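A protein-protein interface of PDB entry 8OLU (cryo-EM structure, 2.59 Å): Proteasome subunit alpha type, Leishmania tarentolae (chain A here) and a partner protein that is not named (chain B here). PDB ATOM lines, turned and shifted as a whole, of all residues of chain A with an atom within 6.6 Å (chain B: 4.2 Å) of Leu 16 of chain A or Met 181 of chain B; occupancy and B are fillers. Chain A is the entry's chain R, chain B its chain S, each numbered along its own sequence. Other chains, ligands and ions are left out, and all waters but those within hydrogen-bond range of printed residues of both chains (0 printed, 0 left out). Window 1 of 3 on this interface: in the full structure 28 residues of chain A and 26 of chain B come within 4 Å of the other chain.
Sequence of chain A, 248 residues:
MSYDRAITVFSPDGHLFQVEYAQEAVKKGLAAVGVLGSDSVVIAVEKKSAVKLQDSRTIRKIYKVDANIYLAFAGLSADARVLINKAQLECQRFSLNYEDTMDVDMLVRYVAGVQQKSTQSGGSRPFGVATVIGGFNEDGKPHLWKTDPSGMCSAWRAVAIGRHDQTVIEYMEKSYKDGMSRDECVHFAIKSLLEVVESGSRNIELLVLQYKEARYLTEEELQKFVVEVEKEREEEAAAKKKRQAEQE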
ATOM      1  N   THR A   8      17.525 -16.048  -9.372  1.00  0.00           N
ATOM      2  CA  THR A   8      16.931 -17.149  -8.661  1.00  0.00           C
ATOM      3  C   THR A   8      15.462 -17.236  -9.061  1.00  0.00           C
ATOM      4  O   THR A   8      14.682 -16.346  -8.727  1.00  0.00           O
ATOM      5  CB  THR A   8      17.105 -16.943  -7.147  1.00  0.00           C
ATOM      6  OG1 THR A   8      18.439 -16.537  -6.804  1.00  0.00           O
ATOM      7  CG2 THR A   8      16.766 -18.201  -6.367  1.00  0.00           C
ATOM      8  N   VAL A   9      15.086 -18.333  -9.717  1.00  0.00           N
ATOM      9  CA  VAL A   9      13.719 -18.508 -10.179  1.00  0.00           C
ATOM     10  C   VAL A   9      13.313 -19.953 -10.022  1.00  0.00           C
ATOM     11  O   VAL A   9      14.156 -20.839 -10.051  1.00  0.00           O
ATOM     12  CB  VAL A   9      13.620 -18.129 -11.664  1.00  0.00           C
ATOM     13  CG1 VAL A   9      13.963 -16.678 -11.861  1.00  0.00           C
ATOM     14  CG2 VAL A   9      14.538 -18.948 -12.539  1.00  0.00           C
ATOM     15  N   PHE A  10      12.026 -20.207  -9.904  1.00  0.00           N
ATOM     16  CA  PHE A  10      11.593 -21.580  -9.795  1.00  0.00           C
ATOM     17  C   PHE A  10      11.734 -22.169 -11.159  1.00  0.00           C
ATOM     18  O   PHE A  10      11.547 -21.456 -12.141  1.00  0.00           O
ATOM     19  CB  PHE A  10      10.129 -21.726  -9.472  1.00  0.00           C
ATOM     20  CG  PHE A  10       9.869 -21.332  -8.072  1.00  0.00           C
ATOM     21  CD1 PHE A  10      10.067 -22.229  -7.065  1.00  0.00           C
ATOM     22  CD2 PHE A  10       9.610 -20.017  -7.776  1.00  0.00           C
ATOM     23  CE1 PHE A  10       9.896 -21.836  -5.758  1.00  0.00           C
ATOM     24  CE2 PHE A  10       9.500 -19.606  -6.465  1.00  0.00           C
ATOM     25  CZ  PHE A  10       9.620 -20.531  -5.462  1.00  0.00           C
ATOM     26  N   SER A  11      12.174 -23.414 -11.150  1.00  0.00           N
ATOM     27  CA  SER A  11      12.171 -24.269 -12.316  1.00  0.00           C
ATOM     28  C   SER A  11      10.865 -25.008 -12.231  1.00  0.00           C
ATOM     29  O   SER A  11      10.203 -24.849 -11.216  1.00  0.00           O
ATOM     30  CB  SER A  11      13.287 -25.268 -12.229  1.00  0.00           C
ATOM     31  OG  SER A  11      12.934 -26.288 -11.264  1.00  0.00           O
ATOM     32  N   GLY A  14       9.326 -27.229  -8.849  1.00  0.00           N
ATOM     33  CA  GLY A  14       9.310 -26.523  -7.580  1.00  0.00           C
ATOM     34  C   GLY A  14      10.676 -26.019  -7.093  1.00  0.00           C
ATOM     35  O   GLY A  14      10.760 -25.318  -6.077  1.00  0.00           O
ATOM     36  N   HIS A  15      11.759 -26.363  -7.796  1.00  0.00           N
ATOM     37  CA  HIS A  15      13.081 -26.130  -7.234  1.00  0.00           C
ATOM     38  C   HIS A  15      13.593 -24.742  -7.584  1.00  0.00           C
ATOM     39  O   HIS A  15      13.333 -24.251  -8.669  1.00  0.00           O
ATOM     40  CB  HIS A  15      14.079 -27.169  -7.758  1.00  0.00           C
ATOM     41  CG  HIS A  15      13.699 -28.584  -7.476  1.00  0.00           C
ATOM     42  ND1 HIS A  15      13.568 -29.533  -8.460  1.00  0.00           N
ATOM     43  CD2 HIS A  15      13.425 -29.164  -6.265  1.00  0.00           C
ATOM     44  CE1 HIS A  15      13.221 -30.680  -7.881  1.00  0.00           C
ATOM     45  NE2 HIS A  15      13.124 -30.474  -6.517  1.00  0.00           N
ATOM     46  N   LEU A  16      14.404 -24.189  -6.699  1.00  0.00           N
ATOM     47  CA  LEU A  16      15.178 -23.007  -6.993  1.00  0.00           C
ATOM     48  C   LEU A  16      16.625 -23.380  -7.281  1.00  0.00           C
ATOM     49  O   LEU A  16      17.474 -23.284  -6.406  1.00  0.00           O
ATOM     50  CB  LEU A  16      15.151 -22.107  -5.760  1.00  0.00           C
ATOM     51  CG  LEU A  16      13.816 -21.496  -5.387  1.00  0.00           C
ATOM     52  CD1 LEU A  16      13.984 -20.517  -4.237  1.00  0.00           C
ATOM     53  CD2 LEU A  16      13.227 -20.751  -6.566  1.00  0.00           C
ATOM     54  N   PHE A  17      16.937 -23.691  -8.528  1.00  0.00           N
ATOM     55  CA  PHE A  17      18.262 -24.154  -8.890  1.00  0.00           C
ATOM     56  C   PHE A  17      19.377 -23.300  -8.302  1.00  0.00           C
ATOM     57  O   PHE A  17      20.307 -23.811  -7.731  1.00  0.00           O
ATOM     58  CB  PHE A  17      18.336 -24.251 -10.406  1.00  0.00           C
ATOM     59  CG  PHE A  17      17.690 -25.494 -10.976  1.00  0.00           C
ATOM     60  CD1 PHE A  17      17.471 -26.616 -10.186  1.00  0.00           C
ATOM     61  CD2 PHE A  17      17.322 -25.539 -12.315  1.00  0.00           C
ATOM     62  CE1 PHE A  17      16.906 -27.760 -10.716  1.00  0.00           C
ATOM     63  CE2 PHE A  17      16.737 -26.681 -12.839  1.00  0.00           C
ATOM     64  CZ  PHE A  17      16.522 -27.782 -12.038  1.00  0.00           C
ATOM     65  N   GLN A  18      19.311 -22.004  -8.380  1.00  0.00           N
ATOM     66  CA  GLN A  18      20.417 -21.254  -7.844  1.00  0.00           C
ATOM     67  C   GLN A  18      20.644 -21.522  -6.367  1.00  0.00           C
ATOM     68  O   GLN A  18      21.732 -21.262  -5.868  1.00  0.00           O
ATOM     69  CB  GLN A  18      20.182 -19.751  -7.951  1.00  0.00           C
ATOM     70  CG  GLN A  18      20.404 -19.213  -9.372  1.00  0.00           C
ATOM     71  CD  GLN A  18      21.775 -19.589  -9.815  1.00  0.00           C
ATOM     72  OE1 GLN A  18      22.720 -18.981  -9.335  1.00  0.00           O
ATOM     73  NE2 GLN A  18      21.871 -20.632 -10.634  1.00  0.00           N
ATOM     74  N   VAL A  19      19.609 -21.959  -5.648  1.00  0.00           N
ATOM     75  CA  VAL A  19      19.731 -22.215  -4.232  1.00  0.00           C
ATOM     76  C   VAL A  19      20.193 -23.630  -4.057  1.00  0.00           C
ATOM     77  O   VAL A  19      20.871 -23.902  -3.098  1.00  0.00           O
ATOM     78  CB  VAL A  19      18.419 -21.946  -3.486  1.00  0.00           C
ATOM     79  CG1 VAL A  19      18.440 -22.506  -2.079  1.00  0.00           C
ATOM     80  CG2 VAL A  19      18.115 -20.456  -3.403  1.00  0.00           C
ATOM     81  N   GLU A  20      19.802 -24.533  -4.946  1.00  0.00           N
ATOM     82  CA  GLU A  20      20.331 -25.878  -4.895  1.00  0.00           C
ATOM     83  C   GLU A  20      21.819 -25.867  -5.227  1.00  0.00           C
ATOM     84  O   GLU A  20      22.569 -26.730  -4.801  1.00  0.00           O
ATOM     85  CB  GLU A  20      19.586 -26.792  -5.850  1.00  0.00           C
ATOM     86  CG  GLU A  20      18.121 -27.026  -5.491  1.00  0.00           C
ATOM     87  CD  GLU A  20      17.551 -28.352  -6.029  1.00  0.00           C
ATOM     88  OE1 GLU A  20      17.601 -28.584  -7.280  1.00  0.00           O
ATOM     89  OE2 GLU A  20      17.068 -29.185  -5.203  1.00  0.00           O
ATOM     90  N   TYR A  21      22.249 -24.892  -5.995  1.00  0.00           N
ATOM     91  CA  TYR A  21      23.619 -24.902  -6.450  1.00  0.00           C
ATOM     92  C   TYR A  21      24.484 -24.168  -5.447  1.00  0.00           C
ATOM     93  O   TYR A  21      25.588 -24.593  -5.145  1.00  0.00           O
ATOM     94  CB  TYR A  21      23.799 -24.241  -7.815  1.00  0.00           C
ATOM     95  CG  TYR A  21      23.079 -24.856  -8.992  1.00  0.00           C
ATOM     96  CD1 TYR A  21      22.732 -26.196  -9.034  1.00  0.00           C
ATOM     97  CD2 TYR A  21      22.730 -24.058 -10.083  1.00  0.00           C
ATOM     98  CE1 TYR A  21      22.088 -26.730 -10.143  1.00  0.00           C
ATOM     99  CE2 TYR A  21      22.079 -24.579 -11.191  1.00  0.00           C
ATOM    100  CZ  TYR A  21      21.744 -25.919 -11.219  1.00  0.00           C
ATOM    101  OH  TYR A  21      21.063 -26.407 -12.322  1.00  0.00           O
ATOM    102  N   THR A 119      18.124 -14.839  -2.160  1.00  0.00           N
ATOM    103  CA  THR A 119      17.516 -15.792  -3.073  1.00  0.00           C
ATOM    104  C   THR A 119      16.312 -15.179  -3.756  1.00  0.00           C
ATOM    105  O   THR A 119      15.577 -15.881  -4.419  1.00  0.00           O
ATOM    106  CB  THR A 119      17.024 -17.014  -2.305  1.00  0.00           C
ATOM    107  OG1 THR A 119      15.859 -16.646  -1.550  1.00  0.00           O
ATOM    108  CG2 THR A 119      18.093 -17.490  -1.365  1.00  0.00           C
ATOM    109  N   MET A 152      17.214 -20.572   5.636  1.00  0.00           N
ATOM    110  CA  MET A 152      16.600 -21.317   6.703  1.00  0.00           C
ATOM    111  C   MET A 152      17.574 -21.494   7.860  1.00  0.00           C
ATOM    112  O   MET A 152      18.609 -22.108   7.716  1.00  0.00           O
ATOM    113  CB  MET A 152      16.218 -22.702   6.215  1.00  0.00           C
ATOM    114  CG  MET A 152      15.391 -23.439   7.203  1.00  0.00           C
ATOM    115  SD  MET A 152      14.500 -24.760   6.322  1.00  0.00           S
ATOM    116  CE  MET A 152      15.567 -26.160   6.687  1.00  0.00           C
ATOM    117  N   GLY B 180       6.105 -24.943   2.585  1.00  0.00           N
ATOM    118  CA  GLY B 180       6.969 -24.747   1.451  1.00  0.00           C
ATOM    119  C   GLY B 180       8.300 -24.265   1.986  1.00  0.00           C
ATOM    120  O   GLY B 180       8.838 -24.765   2.972  1.00  0.00           O
ATOM    121  N   MET B 181       8.744 -23.175   1.420  1.00  0.00           N
ATOM    122  CA  MET B 181      10.039 -22.651   1.745  1.00  0.00           C
ATOM    123  C   MET B 181       9.936 -21.821   2.996  1.00  0.00           C
ATOM    124  O   MET B 181       9.461 -20.703   3.008  1.00  0.00           O
ATOM    125  CB  MET B 181      10.494 -21.807   0.566  1.00  0.00           C
ATOM    126  CG  MET B 181      10.604 -22.667  -0.632  1.00  0.00           C
ATOM    127  SD  MET B 181      11.159 -21.709  -1.987  1.00  0.00           S
ATOM    128  CE  MET B 181      11.681 -23.124  -2.971  1.00  0.00           C
ATOM    129  N   VAL B 182      10.466 -22.365   4.047  1.00  0.00           N
ATOM    130  CA  VAL B 182      10.242 -21.757   5.324  1.00  0.00           C
ATOM    131  C   VAL B 182      10.783 -20.346   5.360  1.00  0.00           C
ATOM    132  O   VAL B 182      10.171 -19.495   5.976  1.00  0.00           O
ATOM    133  CB  VAL B 182      10.876 -22.620   6.411  1.00  0.00           C
ATOM    134  CG1 VAL B 182      10.762 -21.927   7.756  1.00  0.00           C
ATOM    135  CG2 VAL B 182      10.197 -23.992   6.433  1.00  0.00           C
ATOM    136  N   ALA B 183      11.969 -20.110   4.809  1.00  0.00           N
ATOM    137  CA  ALA B 183      12.566 -18.789   4.920  1.00  0.00           C
ATOM    138  C   ALA B 183      11.692 -17.749   4.232  1.00  0.00           C
ATOM    139  O   ALA B 183      11.642 -16.603   4.662  1.00  0.00           O
ATOM    140  CB  ALA B 183      13.889 -18.809   4.260  1.00  0.00           C
ATOM    141  N   ASP B 184      11.024 -18.169   3.144  1.00  0.00           N
ATOM    142  CA  ASP B 184      10.106 -17.296   2.444  1.00  0.00           C
ATOM    143  C   ASP B 184       8.935 -16.996   3.363  1.00  0.00           C
ATOM    144  O   ASP B 184       8.479 -15.858   3.459  1.00  0.00           O
ATOM    145  CB  ASP B 184       9.740 -17.878   1.067  1.00  0.00           C
ATOM    146  CG  ASP B 184      10.849 -17.758   0.001  1.00  0.00           C
ATOM    147  OD1 ASP B 184      11.761 -16.862   0.162  1.00  0.00           O
ATOM    148  OD2 ASP B 184      10.822 -18.554  -1.003  1.00  0.00           O
ATOM    149  N   ALA B 185       8.522 -17.972   4.133  1.00  0.00           N
ATOM    150  CA  ALA B 185       7.417 -17.744   5.026  1.00  0.00           C
ATOM    151  C   ALA B 185       7.730 -16.787   6.149  1.00  0.00           C
ATOM    152  O   ALA B 185       6.832 -16.087   6.614  1.00  0.00           O
ATOM    153  CB  ALA B 185       6.968 -19.046   5.626  1.00  0.00           C
ATOM    154  N   ARG B 235      11.287 -13.392  -7.746  1.00  0.00           N
ATOM    155  CA  ARG B 235      10.424 -14.551  -7.972  1.00  0.00           C
ATOM    156  C   ARG B 235       9.308 -14.542  -6.946  1.00  0.00           C
ATOM    157  O   ARG B 235       9.405 -13.833  -5.965  1.00  0.00           O
ATOM    158  CB  ARG B 235      11.137 -15.878  -7.692  1.00  0.00           C
ATOM    159  CG  ARG B 235      11.905 -15.861  -6.374  1.00  0.00           C
ATOM    160  CD  ARG B 235      12.377 -17.224  -5.937  1.00  0.00           C
ATOM    161  NE  ARG B 235      13.094 -17.076  -4.675  1.00  0.00           N
ATOM    162  CZ  ARG B 235      12.571 -17.370  -3.496  1.00  0.00           C
ATOM    163  NH1 ARG B 235      11.313 -17.802  -3.385  1.00  0.00           N
ATOM    164  NH2 ARG B 235      13.339 -17.207  -2.447  1.00  0.00           N
ATOM    165  N   GLY B 238       7.707 -19.195  -2.367  1.00  0.00           N
ATOM    166  CA  GLY B 238       7.273 -20.561  -2.570  1.00  0.00           C
ATOM    167  C   GLY B 238       6.538 -21.054  -1.339  1.00  0.00           C
ATOM    168  O   GLY B 238       6.949 -22.024  -0.732  1.00  0.00           O
ATOM    169  N   VAL B 239       5.488 -20.357  -0.957  1.00  0.00           N
ATOM    170  CA  VAL B 239       4.942 -20.569   0.365  1.00  0.00           C
ATOM    171  C   VAL B 239       3.444 -20.462   0.272  1.00  0.00           C
ATOM    172  O   VAL B 239       2.940 -19.470  -0.245  1.00  0.00           O
ATOM    173  CB  VAL B 239       5.279 -19.437   1.334  1.00  0.00           C
ATOM    174  CG1 VAL B 239       4.748 -19.779   2.689  1.00  0.00           C
ATOM    175  CG2 VAL B 239       6.729 -19.112   1.437  1.00  0.00           C
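The side-chain hydroxyl (OG1) of Thr 119 of chain A lies within hydrogen-bond range of the guanidinium group (NH2) of Arg 235 of chain B, at 2.7 Å.
OD2 of Asp 184 of chain B lies within hydrogen-bond range of N of Gly 238 of chain B. NH1 of Arg 235 of chain B is in salt-bridge range of OD2 of Asp 184 of chain B (2.5 Å). N of Met 181 of chain B is in hydrogen-bond range of O of Gly 238 of chain B (3.0 Å).
CG of Arg 235 of chain B touches O of Thr 8 of chain A, at 3.7 Å. Met 181 of chain B touches Phe 10 of chain A (CE to CE1, 3.6 Å). Arg 235 of chain B touches Phe 10 of chain A (CD to CE2, 3.8 Å). Phe 10 of chain A touches Gly 238 of chain B. Met 181 of chain B touches Gly 14 of chain A (CE to O, 3.9 Å). Leu 16 of chain A touches Met 181 of chain B. Leu 16 of chain A touches Arg 235 of chain B.
Of the printed residues of chain B, Thr 8 of chain A touches Arg 235 (3.7 Å). Printed residues of chain B within 4 Å of Gly 14 of chain A: Met 181 (3.9 Å). Leu 16 of chain A touches two residues of chain B. Of the printed residues of chain B, Thr 119 of chain A touches Arg 235 (2.7 Å). Printed residues of chain A within 4 Å of Arg 235 of chain B: Thr 8 (3.7 Å), Phe 10 (3.8 Å), Leu 16 (3.5 Å) and Thr 119 (2.7 Å). Of the printed residues of chain A, Gly 238 of chain B touches Phe 10. The nearest printed residue of chain B that does not touch Leu 16 of chain A is Asp 184 of chain B (4.9 Å). The nearest residue of chain A that does not touch Met 181 of chain B is His 15 of chain A (5.2 Å).
Along chain A the printed residues that touch a printed residue of chain B span positions 8 to 119. Printed residues of chain B that touch a printed residue of chain A: Met 181, Arg 235 and Gly 238. Hydrophobic or aromatic side chains of chain B that line the printed part of chain A: Met 181. Among the printed residues, no Asp or Glu carboxylate lies within 4 Å of a Lys or Arg side-chain nitrogen of the other chain.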
